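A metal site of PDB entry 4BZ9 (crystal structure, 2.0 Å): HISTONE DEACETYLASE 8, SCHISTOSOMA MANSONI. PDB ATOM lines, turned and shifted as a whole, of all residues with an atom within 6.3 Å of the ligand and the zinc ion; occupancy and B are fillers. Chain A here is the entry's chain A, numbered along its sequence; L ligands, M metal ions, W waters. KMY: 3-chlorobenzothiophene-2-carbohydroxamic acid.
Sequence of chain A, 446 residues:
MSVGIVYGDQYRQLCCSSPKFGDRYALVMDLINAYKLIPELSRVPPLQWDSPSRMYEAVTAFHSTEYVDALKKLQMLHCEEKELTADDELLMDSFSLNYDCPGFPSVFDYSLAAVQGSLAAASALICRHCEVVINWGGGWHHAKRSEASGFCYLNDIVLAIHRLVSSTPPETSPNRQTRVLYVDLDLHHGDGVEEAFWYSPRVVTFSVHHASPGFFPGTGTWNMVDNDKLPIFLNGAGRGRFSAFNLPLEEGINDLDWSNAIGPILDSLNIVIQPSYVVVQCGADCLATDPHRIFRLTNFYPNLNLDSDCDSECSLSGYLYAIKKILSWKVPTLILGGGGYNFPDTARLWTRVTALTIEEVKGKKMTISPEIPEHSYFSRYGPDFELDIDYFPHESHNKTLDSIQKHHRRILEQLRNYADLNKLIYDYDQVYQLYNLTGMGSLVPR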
ATOM      1  N   LYS A  20      19.935 -15.629 -31.470  1.00  0.00           N
ATOM      2  CA  LYS A  20      19.893 -14.574 -30.451  1.00  0.00           C
ATOM      3  C   LYS A  20      19.780 -13.160 -31.021  1.00  0.00           C
ATOM      4  O   LYS A  20      18.981 -12.369 -30.506  1.00  0.00           O
ATOM      5  CB  LYS A  20      21.138 -14.669 -29.569  1.00  0.00           C
ATOM      6  CG  LYS A  20      21.029 -13.898 -28.275  1.00  0.00           C
ATOM      7  CD  LYS A  20      20.471 -14.787 -27.163  1.00  0.00           C
ATOM      8  CE  LYS A  20      20.575 -14.102 -25.830  1.00  0.00           C
ATOM      9  NZ  LYS A  20      21.914 -13.474 -25.661  1.00  0.00           N
ATOM     10  N   PHE A  21      20.645 -12.808 -31.996  1.00  0.00           N
ATOM     11  CA  PHE A  21      20.613 -11.468 -32.553  1.00  0.00           C
ATOM     12  C   PHE A  21      19.777 -11.302 -33.792  1.00  0.00           C
ATOM     13  O   PHE A  21      19.605 -10.181 -34.266  1.00  0.00           O
ATOM     14  CB  PHE A  21      22.006 -10.820 -32.639  1.00  0.00           C
ATOM     15  CG  PHE A  21      22.603 -10.549 -31.283  1.00  0.00           C
ATOM     16  CD1 PHE A  21      22.176  -9.451 -30.524  1.00  0.00           C
ATOM     17  CD2 PHE A  21      23.532 -11.425 -30.724  1.00  0.00           C
ATOM     18  CE1 PHE A  21      22.687  -9.237 -29.249  1.00  0.00           C
ATOM     19  CE2 PHE A  21      24.043 -11.196 -29.447  1.00  0.00           C
ATOM     20  CZ  PHE A  21      23.638 -10.106 -28.727  1.00  0.00           C
ATOM     21  N   ASP A 100      24.395 -20.668 -22.852  1.00  0.00           N
ATOM     22  CA  ASP A 100      24.357 -19.293 -23.403  1.00  0.00           C
ATOM     23  C   ASP A 100      24.929 -19.215 -24.796  1.00  0.00           C
ATOM     24  O   ASP A 100      24.608 -18.268 -25.523  1.00  0.00           O
ATOM     25  CB  ASP A 100      25.171 -18.317 -22.518  1.00  0.00           C
ATOM     26  CG  ASP A 100      24.633 -18.057 -21.125  1.00  0.00           C
ATOM     27  OD1 ASP A 100      23.396 -18.082 -20.946  1.00  0.00           O
ATOM     28  OD2 ASP A 100      25.455 -17.726 -20.219  1.00  0.00           O
ATOM     29  N   CYS A 101      25.867 -20.147 -25.132  1.00  0.00           N
ATOM     30  CA  CYS A 101      26.545 -20.160 -26.426  1.00  0.00           C
ATOM     31  C   CYS A 101      26.233 -21.456 -27.173  1.00  0.00           C
ATOM     32  O   CYS A 101      27.125 -22.279 -27.372  1.00  0.00           O
ATOM     33  CB  CYS A 101      28.038 -19.954 -26.234  1.00  0.00           C
ATOM     34  SG  CYS A 101      28.450 -18.421 -25.368  1.00  0.00           S
ATOM     35  N   GLY A 139      32.151  -6.410 -31.830  1.00  0.00           N
ATOM     36  CA  GLY A 139      32.110  -6.044 -30.414  1.00  0.00           C
ATOM     37  C   GLY A 139      31.796  -7.171 -29.442  1.00  0.00           C
ATOM     38  O   GLY A 139      31.204  -6.925 -28.385  1.00  0.00           O
ATOM     39  N   TRP A 140      32.242  -8.398 -29.753  1.00  0.00           N
ATOM     40  CA  TRP A 140      31.991  -9.619 -28.962  1.00  0.00           C
ATOM     41  C   TRP A 140      33.040  -9.831 -27.853  1.00  0.00           C
ATOM     42  O   TRP A 140      33.831 -10.791 -27.830  1.00  0.00           O
ATOM     43  CB  TRP A 140      31.790 -10.811 -29.914  1.00  0.00           C
ATOM     44  CG  TRP A 140      30.730 -10.482 -30.920  1.00  0.00           C
ATOM     45  CD1 TRP A 140      30.912 -10.209 -32.243  1.00  0.00           C
ATOM     46  CD2 TRP A 140      29.367 -10.099 -30.615  1.00  0.00           C
ATOM     47  NE1 TRP A 140      29.723  -9.807 -32.814  1.00  0.00           N
ATOM     48  CE2 TRP A 140      28.758  -9.727 -31.838  1.00  0.00           C
ATOM     49  CE3 TRP A 140      28.605 -10.044 -29.435  1.00  0.00           C
ATOM     50  CZ2 TRP A 140      27.424  -9.292 -31.913  1.00  0.00           C
ATOM     51  CZ3 TRP A 140      27.278  -9.616 -29.509  1.00  0.00           C
ATOM     52  CH2 TRP A 140      26.706  -9.264 -30.739  1.00  0.00           C
ATOM     53  N   HIS A 141      32.962  -8.924 -26.891  1.00  0.00           N
ATOM     54  CA  HIS A 141      33.888  -8.741 -25.815  1.00  0.00           C
ATOM     55  C   HIS A 141      34.016  -9.857 -24.777  1.00  0.00           C
ATOM     56  O   HIS A 141      34.992  -9.852 -24.047  1.00  0.00           O
ATOM     57  CB  HIS A 141      33.694  -7.337 -25.186  1.00  0.00           C
ATOM     58  CG  HIS A 141      32.385  -7.133 -24.478  1.00  0.00           C
ATOM     59  ND1 HIS A 141      32.192  -6.045 -23.630  1.00  0.00           N
ATOM     60  CD2 HIS A 141      31.219  -7.829 -24.551  1.00  0.00           C
ATOM     61  CE1 HIS A 141      30.950  -6.142 -23.196  1.00  0.00           C
ATOM     62  NE2 HIS A 141      30.322  -7.185 -23.732  1.00  0.00           N
ATOM     63  N   HIS A 142      33.082 -10.828 -24.729  1.00  0.00           N
ATOM     64  CA  HIS A 142      33.159 -11.854 -23.674  1.00  0.00           C
ATOM     65  C   HIS A 142      33.959 -13.101 -24.027  1.00  0.00           C
ATOM     66  O   HIS A 142      34.311 -13.863 -23.102  1.00  0.00           O
ATOM     67  CB  HIS A 142      31.750 -12.278 -23.224  1.00  0.00           C
ATOM     68  CG  HIS A 142      30.960 -11.172 -22.594  1.00  0.00           C
ATOM     69  ND1 HIS A 142      31.465 -10.422 -21.549  1.00  0.00           N
ATOM     70  CD2 HIS A 142      29.698 -10.781 -22.849  1.00  0.00           C
ATOM     71  CE1 HIS A 142      30.511  -9.548 -21.248  1.00  0.00           C
ATOM     72  NE2 HIS A 142      29.414  -9.753 -21.991  1.00  0.00           N
ATOM     73  N   SER A 149      31.482 -17.290 -24.385  1.00  0.00           N
ATOM     74  CA  SER A 149      30.848 -16.679 -23.204  1.00  0.00           C
ATOM     75  C   SER A 149      29.914 -15.557 -23.622  1.00  0.00           C
ATOM     76  O   SER A 149      30.279 -14.769 -24.483  1.00  0.00           O
ATOM     77  CB  SER A 149      31.935 -16.121 -22.280  1.00  0.00           C
ATOM     78  OG  SER A 149      31.341 -15.556 -21.120  1.00  0.00           O
ATOM     79  N   GLY A 150      28.732 -15.468 -22.992  1.00  0.00           N
ATOM     80  CA  GLY A 150      27.765 -14.403 -23.262  1.00  0.00           C
ATOM     81  C   GLY A 150      27.425 -14.205 -24.732  1.00  0.00           C
ATOM     82  O   GLY A 150      27.347 -13.076 -25.205  1.00  0.00           O
ATOM     83  N   PHE A 151      27.217 -15.317 -25.462  1.00  0.00           N
ATOM     84  CA  PHE A 151      26.930 -15.345 -26.913  1.00  0.00           C
ATOM     85  C   PHE A 151      28.092 -14.775 -27.751  1.00  0.00           C
ATOM     86  O   PHE A 151      27.912 -14.377 -28.909  1.00  0.00           O
ATOM     87  CB  PHE A 151      25.553 -14.718 -27.272  1.00  0.00           C
ATOM     88  CG  PHE A 151      24.957 -15.335 -28.519  1.00  0.00           C
ATOM     89  CD1 PHE A 151      24.378 -16.603 -28.495  1.00  0.00           C
ATOM     90  CD2 PHE A 151      25.033 -14.664 -29.746  1.00  0.00           C
ATOM     91  CE1 PHE A 151      23.860 -17.185 -29.656  1.00  0.00           C
ATOM     92  CE2 PHE A 151      24.521 -15.254 -30.907  1.00  0.00           C
ATOM     93  CZ  PHE A 151      23.929 -16.506 -30.851  1.00  0.00           C
ATOM     94  N   CYS A 152      29.292 -14.735 -27.154  1.00  0.00           N
ATOM     95  CA  CYS A 152      30.509 -14.333 -27.867  1.00  0.00           C
ATOM     96  C   CYS A 152      31.302 -15.598 -28.049  1.00  0.00           C
ATOM     97  O   CYS A 152      31.632 -16.270 -27.069  1.00  0.00           O
ATOM     98  CB  CYS A 152      31.290 -13.278 -27.089  1.00  0.00           C
ATOM     99  SG  CYS A 152      30.300 -11.838 -26.623  1.00  0.00           S
ATOM    100  N   ASP A 186      29.417  -0.962 -23.042  1.00  0.00           N
ATOM    101  CA  ASP A 186      28.377  -1.978 -22.838  1.00  0.00           C
ATOM    102  C   ASP A 186      27.952  -2.080 -21.356  1.00  0.00           C
ATOM    103  O   ASP A 186      28.731  -1.736 -20.446  1.00  0.00           O
ATOM    104  CB  ASP A 186      28.932  -3.323 -23.316  1.00  0.00           C
ATOM    105  CG  ASP A 186      27.873  -4.349 -23.544  1.00  0.00           C
ATOM    106  OD1 ASP A 186      27.422  -4.968 -22.554  1.00  0.00           O
ATOM    107  OD2 ASP A 186      27.560  -4.635 -24.708  1.00  0.00           O
ATOM    108  N   LEU A 187      26.697  -2.497 -21.123  1.00  0.00           N
ATOM    109  CA  LEU A 187      26.124  -2.702 -19.786  1.00  0.00           C
ATOM    110  C   LEU A 187      26.956  -3.684 -19.019  1.00  0.00           C
ATOM    111  O   LEU A 187      27.094  -3.565 -17.811  1.00  0.00           O
ATOM    112  CB  LEU A 187      24.689  -3.241 -19.927  1.00  0.00           C
ATOM    113  CG  LEU A 187      23.907  -3.537 -18.642  1.00  0.00           C
ATOM    114  CD1 LEU A 187      23.689  -2.279 -17.818  1.00  0.00           C
ATOM    115  CD2 LEU A 187      22.557  -4.177 -18.972  1.00  0.00           C
ATOM    116  N   HIS A 188      27.528  -4.668 -19.724  1.00  0.00           N
ATOM    117  CA  HIS A 188      28.319  -5.733 -19.160  1.00  0.00           C
ATOM    118  C   HIS A 188      29.819  -5.439 -19.199  1.00  0.00           C
ATOM    119  O   HIS A 188      30.306  -4.757 -20.107  1.00  0.00           O
ATOM    120  CB  HIS A 188      28.020  -7.018 -19.933  1.00  0.00           C
ATOM    121  CG  HIS A 188      26.595  -7.447 -19.790  1.00  0.00           C
ATOM    122  ND1 HIS A 188      25.658  -7.180 -20.770  1.00  0.00           N
ATOM    123  CD2 HIS A 188      25.975  -8.075 -18.754  1.00  0.00           C
ATOM    124  CE1 HIS A 188      24.516  -7.694 -20.334  1.00  0.00           C
ATOM    125  NE2 HIS A 188      24.657  -8.253 -19.122  1.00  0.00           N
ATOM    126  N   HIS A 189      30.528  -5.967 -18.213  1.00  0.00           N
ATOM    127  CA  HIS A 189      31.994  -5.858 -18.119  1.00  0.00           C
ATOM    128  C   HIS A 189      32.646  -6.548 -19.301  1.00  0.00           C
ATOM    129  O   HIS A 189      32.287  -7.690 -19.621  1.00  0.00           O
ATOM    130  CB  HIS A 189      32.473  -6.535 -16.816  1.00  0.00           C
ATOM    131  CG  HIS A 189      33.971  -6.560 -16.658  1.00  0.00           C
ATOM    132  ND1 HIS A 189      34.638  -7.734 -16.422  1.00  0.00           N
ATOM    133  CD2 HIS A 189      34.874  -5.551 -16.757  1.00  0.00           C
ATOM    134  CE1 HIS A 189      35.919  -7.400 -16.302  1.00  0.00           C
ATOM    135  NE2 HIS A 189      36.108  -6.108 -16.498  1.00  0.00           N
ATOM    136  N   PHE A 216      25.853 -11.096 -14.706  1.00  0.00           N
ATOM    137  CA  PHE A 216      26.870 -11.488 -15.711  1.00  0.00           C
ATOM    138  C   PHE A 216      27.880 -10.391 -16.072  1.00  0.00           C
ATOM    139  O   PHE A 216      27.414  -9.273 -16.276  1.00  0.00           O
ATOM    140  CB  PHE A 216      26.163 -11.934 -17.021  1.00  0.00           C
ATOM    141  CG  PHE A 216      27.102 -12.582 -18.009  1.00  0.00           C
ATOM    142  CD1 PHE A 216      27.416 -13.932 -17.914  1.00  0.00           C
ATOM    143  CD2 PHE A 216      27.705 -11.829 -19.014  1.00  0.00           C
ATOM    144  CE1 PHE A 216      28.294 -14.525 -18.811  1.00  0.00           C
ATOM    145  CE2 PHE A 216      28.609 -12.426 -19.895  1.00  0.00           C
ATOM    146  CZ  PHE A 216      28.898 -13.758 -19.781  1.00  0.00           C
ATOM    147  N   GLN A 281      33.794  -0.093 -27.612  1.00  0.00           N
ATOM    148  CA  GLN A 281      32.744  -1.109 -27.743  1.00  0.00           C
ATOM    149  C   GLN A 281      31.492  -0.312 -27.345  1.00  0.00           C
ATOM    150  O   GLN A 281      31.500   0.319 -26.293  1.00  0.00           O
ATOM    151  CB  GLN A 281      33.024  -2.330 -26.829  1.00  0.00           C
ATOM    152  CG  GLN A 281      32.178  -3.567 -27.188  1.00  0.00           C
ATOM    153  CD  GLN A 281      30.878  -3.661 -26.433  1.00  0.00           C
ATOM    154  OE1 GLN A 281      30.341  -2.686 -25.899  1.00  0.00           O
ATOM    155  NE2 GLN A 281      30.327  -4.845 -26.355  1.00  0.00           N
ATOM    156  N   GLY A 283      28.066  -1.377 -27.003  1.00  0.00           N
ATOM    157  CA  GLY A 283      26.895  -2.213 -26.729  1.00  0.00           C
ATOM    158  C   GLY A 283      25.754  -1.336 -26.260  1.00  0.00           C
ATOM    159  O   GLY A 283      25.976  -0.446 -25.425  1.00  0.00           O
ATOM    160  N   ASP A 285      22.968  -2.076 -24.616  1.00  0.00           N
ATOM    161  CA  ASP A 285      22.165  -2.631 -23.521  1.00  0.00           C
ATOM    162  C   ASP A 285      22.017  -1.705 -22.321  1.00  0.00           C
ATOM    163  O   ASP A 285      21.277  -2.047 -21.390  1.00  0.00           O
ATOM    164  CB  ASP A 285      22.606  -4.050 -23.142  1.00  0.00           C
ATOM    165  CG  ASP A 285      24.088  -4.330 -23.266  1.00  0.00           C
ATOM    166  OD1 ASP A 285      24.881  -3.343 -23.362  1.00  0.00           O
ATOM    167  OD2 ASP A 285      24.470  -5.517 -23.229  1.00  0.00           O
ATOM    168  N   HIS A 292      16.892  -5.616 -20.306  1.00  0.00           N
ATOM    169  CA  HIS A 292      17.655  -5.770 -19.059  1.00  0.00           C
ATOM    170  C   HIS A 292      17.057  -4.821 -18.023  1.00  0.00           C
ATOM    171  O   HIS A 292      16.902  -5.194 -16.848  1.00  0.00           O
ATOM    172  CB  HIS A 292      19.134  -5.386 -19.262  1.00  0.00           C
ATOM    173  CG  HIS A 292      19.965  -6.453 -19.907  1.00  0.00           C
ATOM    174  ND1 HIS A 292      20.167  -6.482 -21.275  1.00  0.00           N
ATOM    175  CD2 HIS A 292      20.648  -7.470 -19.335  1.00  0.00           C
ATOM    176  CE1 HIS A 292      20.962  -7.524 -21.496  1.00  0.00           C
ATOM    177  NE2 HIS A 292      21.263  -8.153 -20.368  1.00  0.00           N
ATOM    178  N   GLY A 338      27.856  -4.547 -30.082  1.00  0.00           N
ATOM    179  CA  GLY A 338      27.891  -5.376 -28.894  1.00  0.00           C
ATOM    180  C   GLY A 338      26.499  -5.743 -28.513  1.00  0.00           C
ATOM    181  O   GLY A 338      25.704  -6.158 -29.357  1.00  0.00           O
ATOM    182  N   GLY A 339      26.195  -5.591 -27.226  1.00  0.00           N
ATOM    183  CA  GLY A 339      24.897  -5.963 -26.670  1.00  0.00           C
ATOM    184  C   GLY A 339      23.785  -5.068 -27.180  1.00  0.00           C
ATOM    185  O   GLY A 339      24.048  -4.042 -27.819  1.00  0.00           O
ATOM    186  N   GLY A 340      22.560  -5.483 -26.919  1.00  0.00           N
ATOM    187  CA  GLY A 340      21.365  -4.751 -27.302  1.00  0.00           C
ATOM    188  C   GLY A 340      20.319  -5.710 -27.796  1.00  0.00           C
ATOM    189  O   GLY A 340      20.413  -6.174 -28.928  1.00  0.00           O
ATOM    190  N   TYR A 341      19.342  -6.033 -26.933  1.00  0.00           N
ATOM    191  CA  TYR A 341      18.244  -6.943 -27.272  1.00  0.00           C
ATOM    192  C   TYR A 341      17.047  -6.243 -27.890  1.00  0.00           C
ATOM    193  O   TYR A 341      16.237  -6.893 -28.565  1.00  0.00           O
ATOM    194  CB  TYR A 341      17.803  -7.759 -26.047  1.00  0.00           C
ATOM    195  CG  TYR A 341      18.836  -8.730 -25.517  1.00  0.00           C
ATOM    196  CD1 TYR A 341      19.615  -9.488 -26.383  1.00  0.00           C
ATOM    197  CD2 TYR A 341      18.964  -8.953 -24.148  1.00  0.00           C
ATOM    198  CE1 TYR A 341      20.543 -10.408 -25.896  1.00  0.00           C
ATOM    199  CE2 TYR A 341      19.890  -9.875 -23.652  1.00  0.00           C
ATOM    200  CZ  TYR A 341      20.674 -10.601 -24.532  1.00  0.00           C
ATOM    201  OH  TYR A 341      21.577 -11.503 -24.026  1.00  0.00           O
HETATM  202  O01 KMY L   1      25.141  -8.272 -24.238  1.00  0.00           O
HETATM  203  C02 KMY L   1      25.893  -9.042 -23.676  1.00  0.00           C
HETATM  204  N03 KMY L   1      27.223  -8.671 -23.299  1.00  0.00           N
HETATM  205  O04 KMY L   1      27.741  -7.535 -23.612  1.00  0.00           O
HETATM  206  C05 KMY L   1      25.433 -10.384 -23.224  1.00  0.00           C
HETATM  207  S06 KMY L   1      25.783 -10.961 -21.659  1.00  0.00           S
HETATM  208  C07 KMY L   1      25.062 -12.520 -21.805  1.00  0.00           C
HETATM  209  C08 KMY L   1      24.939 -13.589 -20.905  1.00  0.00           C
HETATM  210  C09 KMY L   1      24.280 -14.758 -21.316  1.00  0.00           C
HETATM  211  C10 KMY L   1      23.781 -14.850 -22.627  1.00  0.00           C
HETATM  212  C11 KMY L   1      23.937 -13.792 -23.511  1.00  0.00           C
HETATM  213  C12 KMY L   1      24.589 -12.602 -23.098  1.00  0.00           C
HETATM  214  C13 KMY L   1      24.802 -11.432 -23.886  1.00  0.00           C
HETATM  215 CL   KMY L   1      24.241 -11.338 -25.528  1.00  0.00          CL
HETATM  216 ZN    ZN M   1      26.138  -6.460 -22.796  1.00  0.00          ZN
HETATM  217  O   HOH W   1      22.478  -7.918 -24.924  1.00  0.00           O
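An oxygen (O04) of the ligand lies close to a ring nitrogen (NE2) of His 141, at 2.6 Å. A nitrogen (N03) of the ligand sits close to a ring nitrogen (NE2) of His 142 (2.8 Å).
The side-chain carboxylate (OD1) of Asp 285 sits at hydrogen-bond distance from the backbone NH (N) of Leu 187, 3.0 Å away. The side-chain carboxylate (OD2) of Asp 186 is in hydrogen-bond range of the backbone NH (N) of Gly 339, 3.0 Å away. OD2 of Asp 186 sits at hydrogen-bond distance from NE2 of Gln 281, at 3.2 Å. A ring nitrogen (NE2) of His 142 is in hydrogen-bond range of a ring nitrogen (NE2) of His 141 (3.2 Å). SG of Cys 152 sits at hydrogen-bond distance from N of His 142 (3.5 Å). A ring nitrogen (ND1) of His 142 lies close to the backbone carbonyl oxygen (O) of His 189 (3.4 Å). The side-chain amino group of Lys 20 sits at hydrogen-bond distance from the side-chain hydroxyl of Tyr 341 (2.6 Å). O of Gly 150 lies within hydrogen-bond range of SG of Cys 152 (3.5 Å).
NZ of Lys 20 touches C11 of the ligand (3.0 Å). Phe 21 touches the ligand (CZ to CL, 3.5 Å). CG of Asp 100 touches C09 of the ligand, at 3.3 Å. Gly 150 touches the ligand. Phe 216 touches the ligand. Gly 339 touches the ligand (CA to O01, 3.4 Å). Tyr 341 touches the ligand (OH to CL, 3.1 Å). Hydrophobic or aromatic side chains that line the ligand: Phe 21, His 141, His 142, His 188, Phe 216 and Tyr 341. Of the 25 residues printed, 12 come within 4 Å of the ligand. The nearest printed residue that does not touch the ligand is Phe 151 (4.02 Å).
Of the 25 residues printed, 3 come within 4 Å of the zinc ion.
The zinc ion is bound by the side-chain carboxylate of Asp 285 (2.0 Å), the side-chain carboxylate of Asp 186 (2.0 Å), an oxygen (O04) of the ligand (2.1 Å), a ring nitrogen (ND1) of His 188 (2.2 Å) and an oxygen (O01) of the ligand (2.5 Å).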
